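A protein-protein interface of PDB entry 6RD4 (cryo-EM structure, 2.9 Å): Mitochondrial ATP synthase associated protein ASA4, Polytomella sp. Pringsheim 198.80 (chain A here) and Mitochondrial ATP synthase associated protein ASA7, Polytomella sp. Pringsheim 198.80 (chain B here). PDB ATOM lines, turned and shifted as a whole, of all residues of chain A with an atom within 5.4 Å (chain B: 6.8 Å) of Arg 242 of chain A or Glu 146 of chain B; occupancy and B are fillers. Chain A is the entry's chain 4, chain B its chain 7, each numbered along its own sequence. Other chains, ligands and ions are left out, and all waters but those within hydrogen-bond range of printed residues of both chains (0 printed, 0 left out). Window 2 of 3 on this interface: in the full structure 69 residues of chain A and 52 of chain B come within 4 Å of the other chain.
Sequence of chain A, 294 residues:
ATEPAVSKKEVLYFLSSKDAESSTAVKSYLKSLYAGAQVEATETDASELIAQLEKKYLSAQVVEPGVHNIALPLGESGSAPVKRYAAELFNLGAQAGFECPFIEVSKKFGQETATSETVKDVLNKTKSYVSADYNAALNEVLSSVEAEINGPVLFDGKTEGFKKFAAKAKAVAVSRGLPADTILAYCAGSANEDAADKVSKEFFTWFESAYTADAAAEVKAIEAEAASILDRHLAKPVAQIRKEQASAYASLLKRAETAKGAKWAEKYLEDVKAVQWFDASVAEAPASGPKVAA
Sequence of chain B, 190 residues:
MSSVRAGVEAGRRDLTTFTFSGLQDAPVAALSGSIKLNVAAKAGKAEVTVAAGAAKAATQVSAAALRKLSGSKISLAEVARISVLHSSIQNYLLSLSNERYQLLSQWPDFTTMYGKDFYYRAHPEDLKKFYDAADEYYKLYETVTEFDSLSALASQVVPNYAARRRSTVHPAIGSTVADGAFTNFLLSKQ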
ATOM      1  N   HIS A 233     -16.914 -29.755  -4.759  1.00  0.00           N
ATOM      2  CA  HIS A 233     -16.195 -28.611  -5.296  1.00  0.00           C
ATOM      3  C   HIS A 233     -15.849 -27.604  -4.221  1.00  0.00           C
ATOM      4  O   HIS A 233     -14.820 -26.941  -4.319  1.00  0.00           O
ATOM      5  CB  HIS A 233     -17.044 -27.993  -6.410  1.00  0.00           C
ATOM      6  CG  HIS A 233     -16.750 -26.564  -6.736  1.00  0.00           C
ATOM      7  ND1 HIS A 233     -17.319 -25.517  -6.052  1.00  0.00           N
ATOM      8  CD2 HIS A 233     -16.047 -26.013  -7.746  1.00  0.00           C
ATOM      9  CE1 HIS A 233     -16.924 -24.378  -6.584  1.00  0.00           C
ATOM     10  NE2 HIS A 233     -16.154 -24.651  -7.616  1.00  0.00           N
ATOM     11  N   VAL A 238      -8.922 -23.151  -4.298  1.00  0.00           N
ATOM     12  CA  VAL A 238      -9.355 -22.343  -5.433  1.00  0.00           C
ATOM     13  C   VAL A 238      -8.420 -22.493  -6.615  1.00  0.00           C
ATOM     14  O   VAL A 238      -8.846 -22.388  -7.764  1.00  0.00           O
ATOM     15  CB  VAL A 238      -9.447 -20.881  -4.996  1.00  0.00           C
ATOM     16  CG1 VAL A 238     -10.203 -20.091  -5.968  1.00  0.00           C
ATOM     17  CG2 VAL A 238     -10.096 -20.819  -3.696  1.00  0.00           C
ATOM     18  N   ALA A 239      -7.140 -22.743  -6.365  1.00  0.00           N
ATOM     19  CA  ALA A 239      -6.211 -22.916  -7.468  1.00  0.00           C
ATOM     20  C   ALA A 239      -6.469 -24.211  -8.212  1.00  0.00           C
ATOM     21  O   ALA A 239      -6.213 -24.290  -9.414  1.00  0.00           O
ATOM     22  CB  ALA A 239      -4.784 -22.883  -6.952  1.00  0.00           C
ATOM     23  N   GLN A 240      -6.981 -25.223  -7.520  1.00  0.00           N
ATOM     24  CA  GLN A 240      -7.341 -26.466  -8.184  1.00  0.00           C
ATOM     25  C   GLN A 240      -8.572 -26.277  -9.044  1.00  0.00           C
ATOM     26  O   GLN A 240      -8.648 -26.814 -10.151  1.00  0.00           O
ATOM     27  CB  GLN A 240      -7.584 -27.554  -7.150  1.00  0.00           C
ATOM     28  CG  GLN A 240      -7.930 -28.875  -7.742  1.00  0.00           C
ATOM     29  CD  GLN A 240      -8.207 -29.915  -6.699  1.00  0.00           C
ATOM     30  OE1 GLN A 240      -8.778 -30.961  -6.989  1.00  0.00           O
ATOM     31  NE2 GLN A 240      -7.803 -29.638  -5.469  1.00  0.00           N
ATOM     32  N   ILE A 241      -9.528 -25.489  -8.555  1.00  0.00           N
ATOM     33  CA  ILE A 241     -10.810 -25.307  -9.224  1.00  0.00           C
ATOM     34  C   ILE A 241     -10.631 -24.577 -10.536  1.00  0.00           C
ATOM     35  O   ILE A 241     -11.157 -25.000 -11.568  1.00  0.00           O
ATOM     36  CB  ILE A 241     -11.770 -24.549  -8.300  1.00  0.00           C
ATOM     37  CG1 ILE A 241     -12.245 -25.434  -7.176  1.00  0.00           C
ATOM     38  CG2 ILE A 241     -12.932 -24.029  -9.044  1.00  0.00           C
ATOM     39  CD1 ILE A 241     -13.065 -24.695  -6.214  1.00  0.00           C
ATOM     40  N   ARG A 242      -9.857 -23.494 -10.530  1.00  0.00           N
ATOM     41  CA  ARG A 242      -9.720 -22.661 -11.713  1.00  0.00           C
ATOM     42  C   ARG A 242      -8.976 -23.368 -12.825  1.00  0.00           C
ATOM     43  O   ARG A 242      -9.215 -23.083 -13.997  1.00  0.00           O
ATOM     44  CB  ARG A 242      -8.993 -21.373 -11.370  1.00  0.00           C
ATOM     45  CG  ARG A 242      -9.653 -20.566 -10.322  1.00  0.00           C
ATOM     46  CD  ARG A 242      -9.361 -19.126 -10.529  1.00  0.00           C
ATOM     47  NE  ARG A 242      -9.809 -18.326  -9.408  1.00  0.00           N
ATOM     48  CZ  ARG A 242      -8.995 -17.825  -8.497  1.00  0.00           C
ATOM     49  NH1 ARG A 242      -7.694 -18.049  -8.585  1.00  0.00           N
ATOM     50  NH2 ARG A 242      -9.478 -17.101  -7.505  1.00  0.00           N
ATOM     51  N   LYS A 243      -8.086 -24.291 -12.491  1.00  0.00           N
ATOM     52  CA  LYS A 243      -7.370 -25.023 -13.517  1.00  0.00           C
ATOM     53  C   LYS A 243      -8.019 -26.349 -13.862  1.00  0.00           C
ATOM     54  O   LYS A 243      -7.730 -26.891 -14.925  1.00  0.00           O
ATOM     55  CB  LYS A 243      -5.919 -25.251 -13.098  1.00  0.00           C
ATOM     56  CG  LYS A 243      -5.730 -26.294 -12.032  1.00  0.00           C
ATOM     57  CD  LYS A 243      -4.299 -26.771 -11.993  1.00  0.00           C
ATOM     58  CE  LYS A 243      -3.904 -27.377 -13.320  1.00  0.00           C
ATOM     59  NZ  LYS A 243      -4.869 -28.433 -13.720  1.00  0.00           N
ATOM     60  N   GLU A 244      -8.878 -26.889 -12.997  1.00  0.00           N
ATOM     61  CA  GLU A 244      -9.710 -28.014 -13.409  1.00  0.00           C
ATOM     62  C   GLU A 244     -10.747 -27.566 -14.419  1.00  0.00           C
ATOM     63  O   GLU A 244     -11.088 -28.309 -15.339  1.00  0.00           O
ATOM     64  CB  GLU A 244     -10.415 -28.630 -12.213  1.00  0.00           C
ATOM     65  CG  GLU A 244      -9.672 -29.725 -11.524  1.00  0.00           C
ATOM     66  CD  GLU A 244     -10.542 -30.440 -10.514  1.00  0.00           C
ATOM     67  OE1 GLU A 244     -11.479 -29.808  -9.988  1.00  0.00           O
ATOM     68  OE2 GLU A 244     -10.298 -31.637 -10.256  1.00  0.00           O
ATOM     69  N   GLN A 245     -11.265 -26.359 -14.246  1.00  0.00           N
ATOM     70  CA  GLN A 245     -12.295 -25.846 -15.125  1.00  0.00           C
ATOM     71  C   GLN A 245     -11.731 -25.257 -16.398  1.00  0.00           C
ATOM     72  O   GLN A 245     -12.377 -25.338 -17.440  1.00  0.00           O
ATOM     73  CB  GLN A 245     -13.106 -24.790 -14.404  1.00  0.00           C
ATOM     74  CG  GLN A 245     -13.940 -25.329 -13.302  1.00  0.00           C
ATOM     75  CD  GLN A 245     -14.809 -24.273 -12.739  1.00  0.00           C
ATOM     76  OE1 GLN A 245     -14.569 -23.095 -12.955  1.00  0.00           O
ATOM     77  NE2 GLN A 245     -15.829 -24.673 -12.008  1.00  0.00           N
ATOM     78  N   ALA A 246     -10.558 -24.636 -16.337  1.00  0.00           N
ATOM     79  CA  ALA A 246      -9.927 -24.159 -17.555  1.00  0.00           C
ATOM     80  C   ALA A 246      -9.391 -25.292 -18.400  1.00  0.00           C
ATOM     81  O   ALA A 246      -9.316 -25.151 -19.621  1.00  0.00           O
ATOM     82  CB  ALA A 246      -8.793 -23.200 -17.234  1.00  0.00           C
ATOM     83  N   SER A 247      -9.006 -26.405 -17.778  1.00  0.00           N
ATOM     84  CA  SER A 247      -8.660 -27.596 -18.539  1.00  0.00           C
ATOM     85  C   SER A 247      -9.882 -28.193 -19.206  1.00  0.00           C
ATOM     86  O   SER A 247      -9.805 -28.666 -20.343  1.00  0.00           O
ATOM     87  CB  SER A 247      -8.016 -28.634 -17.635  1.00  0.00           C
ATOM     88  OG  SER A 247      -7.852 -29.854 -18.325  1.00  0.00           O
ATOM     89  N   SER B  97     -24.686 -22.235  -2.434  1.00  0.00           N
ATOM     90  CA  SER B  97     -23.508 -21.552  -1.918  1.00  0.00           C
ATOM     91  C   SER B  97     -23.860 -20.537  -0.864  1.00  0.00           C
ATOM     92  O   SER B  97     -23.025 -20.215  -0.029  1.00  0.00           O
ATOM     93  CB  SER B  97     -22.756 -20.835  -3.015  1.00  0.00           C
ATOM     94  OG  SER B  97     -22.062 -21.743  -3.812  1.00  0.00           O
ATOM     95  N   TYR B 141     -13.289 -20.126   2.775  1.00  0.00           N
ATOM     96  CA  TYR B 141     -13.958 -18.895   2.402  1.00  0.00           C
ATOM     97  C   TYR B 141     -13.576 -18.419   1.019  1.00  0.00           C
ATOM     98  O   TYR B 141     -14.391 -17.800   0.346  1.00  0.00           O
ATOM     99  CB  TYR B 141     -13.648 -17.816   3.414  1.00  0.00           C
ATOM    100  CG  TYR B 141     -14.425 -16.566   3.227  1.00  0.00           C
ATOM    101  CD1 TYR B 141     -15.736 -16.488   3.612  1.00  0.00           C
ATOM    102  CD2 TYR B 141     -13.841 -15.454   2.676  1.00  0.00           C
ATOM    103  CE1 TYR B 141     -16.437 -15.347   3.446  1.00  0.00           C
ATOM    104  CE2 TYR B 141     -14.543 -14.309   2.510  1.00  0.00           C
ATOM    105  CZ  TYR B 141     -15.832 -14.264   2.894  1.00  0.00           C
ATOM    106  OH  TYR B 141     -16.524 -13.111   2.715  1.00  0.00           O
ATOM    107  N   GLU B 142     -12.360 -18.672   0.571  1.00  0.00           N
ATOM    108  CA  GLU B 142     -11.997 -18.226  -0.760  1.00  0.00           C
ATOM    109  C   GLU B 142     -12.554 -19.116  -1.843  1.00  0.00           C
ATOM    110  O   GLU B 142     -12.520 -18.728  -3.005  1.00  0.00           O
ATOM    111  CB  GLU B 142     -10.482 -18.119  -0.904  1.00  0.00           C
ATOM    112  CG  GLU B 142      -9.879 -16.980  -0.097  1.00  0.00           C
ATOM    113  CD  GLU B 142      -8.422 -16.729  -0.409  1.00  0.00           C
ATOM    114  OE1 GLU B 142      -7.675 -17.714  -0.605  1.00  0.00           O
ATOM    115  OE2 GLU B 142      -8.019 -15.543  -0.442  1.00  0.00           O
ATOM    116  N   THR B 143     -13.047 -20.298  -1.508  1.00  0.00           N
ATOM    117  CA  THR B 143     -13.681 -21.139  -2.504  1.00  0.00           C
ATOM    118  C   THR B 143     -15.194 -21.077  -2.467  1.00  0.00           C
ATOM    119  O   THR B 143     -15.821 -21.434  -3.457  1.00  0.00           O
ATOM    120  CB  THR B 143     -13.240 -22.599  -2.370  1.00  0.00           C
ATOM    121  OG1 THR B 143     -13.879 -23.355  -3.386  1.00  0.00           O
ATOM    122  CG2 THR B 143     -13.652 -23.172  -1.094  1.00  0.00           C
ATOM    123  N   VAL B 144     -15.806 -20.626  -1.379  1.00  0.00           N
ATOM    124  CA  VAL B 144     -17.250 -20.498  -1.392  1.00  0.00           C
ATOM    125  C   VAL B 144     -17.648 -19.190  -2.047  1.00  0.00           C
ATOM    126  O   VAL B 144     -18.794 -19.049  -2.485  1.00  0.00           O
ATOM    127  CB  VAL B 144     -17.849 -20.615   0.018  1.00  0.00           C
ATOM    128  CG1 VAL B 144     -17.767 -19.338   0.746  1.00  0.00           C
ATOM    129  CG2 VAL B 144     -19.251 -21.092  -0.030  1.00  0.00           C
ATOM    130  N   THR B 145     -16.726 -18.246  -2.165  1.00  0.00           N
ATOM    131  CA  THR B 145     -16.972 -16.993  -2.838  1.00  0.00           C
ATOM    132  C   THR B 145     -16.414 -17.002  -4.237  1.00  0.00           C
ATOM    133  O   THR B 145     -16.377 -15.967  -4.885  1.00  0.00           O
ATOM    134  CB  THR B 145     -16.400 -15.844  -2.038  1.00  0.00           C
ATOM    135  OG1 THR B 145     -14.992 -15.999  -1.944  1.00  0.00           O
ATOM    136  CG2 THR B 145     -16.951 -15.878  -0.674  1.00  0.00           C
ATOM    137  N   GLU B 146     -16.008 -18.157  -4.725  1.00  0.00           N
ATOM    138  CA  GLU B 146     -15.647 -18.335  -6.122  1.00  0.00           C
ATOM    139  C   GLU B 146     -16.935 -18.612  -6.887  1.00  0.00           C
ATOM    140  O   GLU B 146     -17.247 -19.739  -7.264  1.00  0.00           O
ATOM    141  CB  GLU B 146     -14.639 -19.462  -6.250  1.00  0.00           C
ATOM    142  CG  GLU B 146     -14.048 -19.674  -7.598  1.00  0.00           C
ATOM    143  CD  GLU B 146     -13.160 -18.568  -8.027  1.00  0.00           C
ATOM    144  OE1 GLU B 146     -12.478 -17.997  -7.163  1.00  0.00           O
ATOM    145  OE2 GLU B 146     -13.124 -18.260  -9.232  1.00  0.00           O
ATOM    146  N   PHE B 147     -17.714 -17.557  -7.096  1.00  0.00           N
ATOM    147  CA  PHE B 147     -19.001 -17.694  -7.754  1.00  0.00           C
ATOM    148  C   PHE B 147     -18.892 -17.753  -9.260  1.00  0.00           C
ATOM    149  O   PHE B 147     -19.888 -18.045  -9.917  1.00  0.00           O
ATOM    150  CB  PHE B 147     -19.917 -16.537  -7.404  1.00  0.00           C
ATOM    151  CG  PHE B 147     -20.145 -16.352  -5.956  1.00  0.00           C
ATOM    152  CD1 PHE B 147     -20.745 -17.318  -5.214  1.00  0.00           C
ATOM    153  CD2 PHE B 147     -19.788 -15.185  -5.346  1.00  0.00           C
ATOM    154  CE1 PHE B 147     -20.973 -17.117  -3.890  1.00  0.00           C
ATOM    155  CE2 PHE B 147     -20.022 -14.987  -4.037  1.00  0.00           C
ATOM    156  CZ  PHE B 147     -20.604 -15.952  -3.309  1.00  0.00           C
ATOM    157  N   ASP B 148     -17.735 -17.471  -9.834  1.00  0.00           N
ATOM    158  CA  ASP B 148     -17.530 -17.672 -11.254  1.00  0.00           C
ATOM    159  C   ASP B 148     -17.275 -19.122 -11.599  1.00  0.00           C
ATOM    160  O   ASP B 148     -17.102 -19.448 -12.772  1.00  0.00           O
ATOM    161  CB  ASP B 148     -16.364 -16.837 -11.750  1.00  0.00           C
ATOM    162  CG  ASP B 148     -16.722 -15.391 -11.931  1.00  0.00           C
ATOM    163  OD1 ASP B 148     -17.858 -15.008 -11.601  1.00  0.00           O
ATOM    164  OD2 ASP B 148     -15.860 -14.628 -12.410  1.00  0.00           O
ATOM    165  N   SER B 149     -17.233 -19.996 -10.610  1.00  0.00           N
ATOM    166  CA  SER B 149     -17.126 -21.417 -10.842  1.00  0.00           C
ATOM    167  C   SER B 149     -18.459 -22.123 -10.804  1.00  0.00           C
ATOM    168  O   SER B 149     -18.515 -23.310 -11.107  1.00  0.00           O
ATOM    169  CB  SER B 149     -16.202 -22.033  -9.817  1.00  0.00           C
ATOM    170  OG  SER B 149     -14.891 -21.596 -10.070  1.00  0.00           O
ATOM    171  N   LEU B 150     -19.526 -21.433 -10.423  1.00  0.00           N
ATOM    172  CA  LEU B 150     -20.818 -22.083 -10.373  1.00  0.00           C
ATOM    173  C   LEU B 150     -21.422 -22.254 -11.747  1.00  0.00           C
ATOM    174  O   LEU B 150     -22.261 -23.128 -11.927  1.00  0.00           O
ATOM    175  CB  LEU B 150     -21.766 -21.298  -9.489  1.00  0.00           C
ATOM    176  CG  LEU B 150     -21.301 -21.142  -8.063  1.00  0.00           C
ATOM    177  CD1 LEU B 150     -22.325 -20.407  -7.322  1.00  0.00           C
ATOM    178  CD2 LEU B 150     -21.107 -22.465  -7.460  1.00  0.00           C
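Arg 242 of chain A touches one residue of chain B. Printed residues of chain A within 4 Å of Glu 146 of chain B: Val 238 and Arg 242. Printed residues of chain A within 4 Å of Thr 143 of chain B: His 233 (3.8 Å), Val 238 (3.7 Å) and Ile 241 (3.2 Å). Of the printed residues of chain B, Val 238 of chain A touches Glu 142, Thr 143 and Glu 146. Of the printed residues of chain A, Glu 142 of chain B touches Val 238 (3.3 Å). Printed residues of chain B within 4 Å of Gln 245 of chain A: Ser 149. Printed residues of chain A within 4 Å of Ser 149 of chain B: His 233 (3.4 Å), Ile 241 (3.3 Å) and Gln 245 (3.1 Å). Asp 148 of chain B touches none of the printed residues of chain A. The nearest printed residue of chain B that does not touch Ile 241 of chain A is Glu 146 of chain B (4.7 Å).
Of the 11 printed residues of chain A, 5 touch a printed residue of chain B. Printed residues of chain A that touch a printed residue of chain B: His 233, Val 238, Ile 241, Arg 242 and Gln 245. Along chain B the printed residues that touch a printed residue of chain A span positions 142 to 149. Among the printed residues, 9 pairs touch across the chains.
His 233 of chain A touches Thr 143 of chain B. His 233 of chain A touches Ser 149 of chain B (NE2 to CB, 3.4 Å). Val 238 of chain A touches Glu 142 of chain B (CG2 to O, 3.3 Å). Thr 143 of chain B touches Val 238 of chain A (N to CG2, 3.7 Å). Val 238 of chain A touches Glu 146 of chain B. Ile 241 of chain A touches Thr 143 of chain B. Ile 241 of chain A touches Ser 149 of chain B (CG2 to OG, 3.3 Å).
OE1 of Glu 146 of chain B lies within salt-bridge range of NH2 of Arg 242 of chain A (3.1 Å). The side-chain amide nitrogen of Gln 245 of chain A is in hydrogen-bond range of the backbone carbonyl oxygen of Ser 149 of chain B (3.1 Å).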
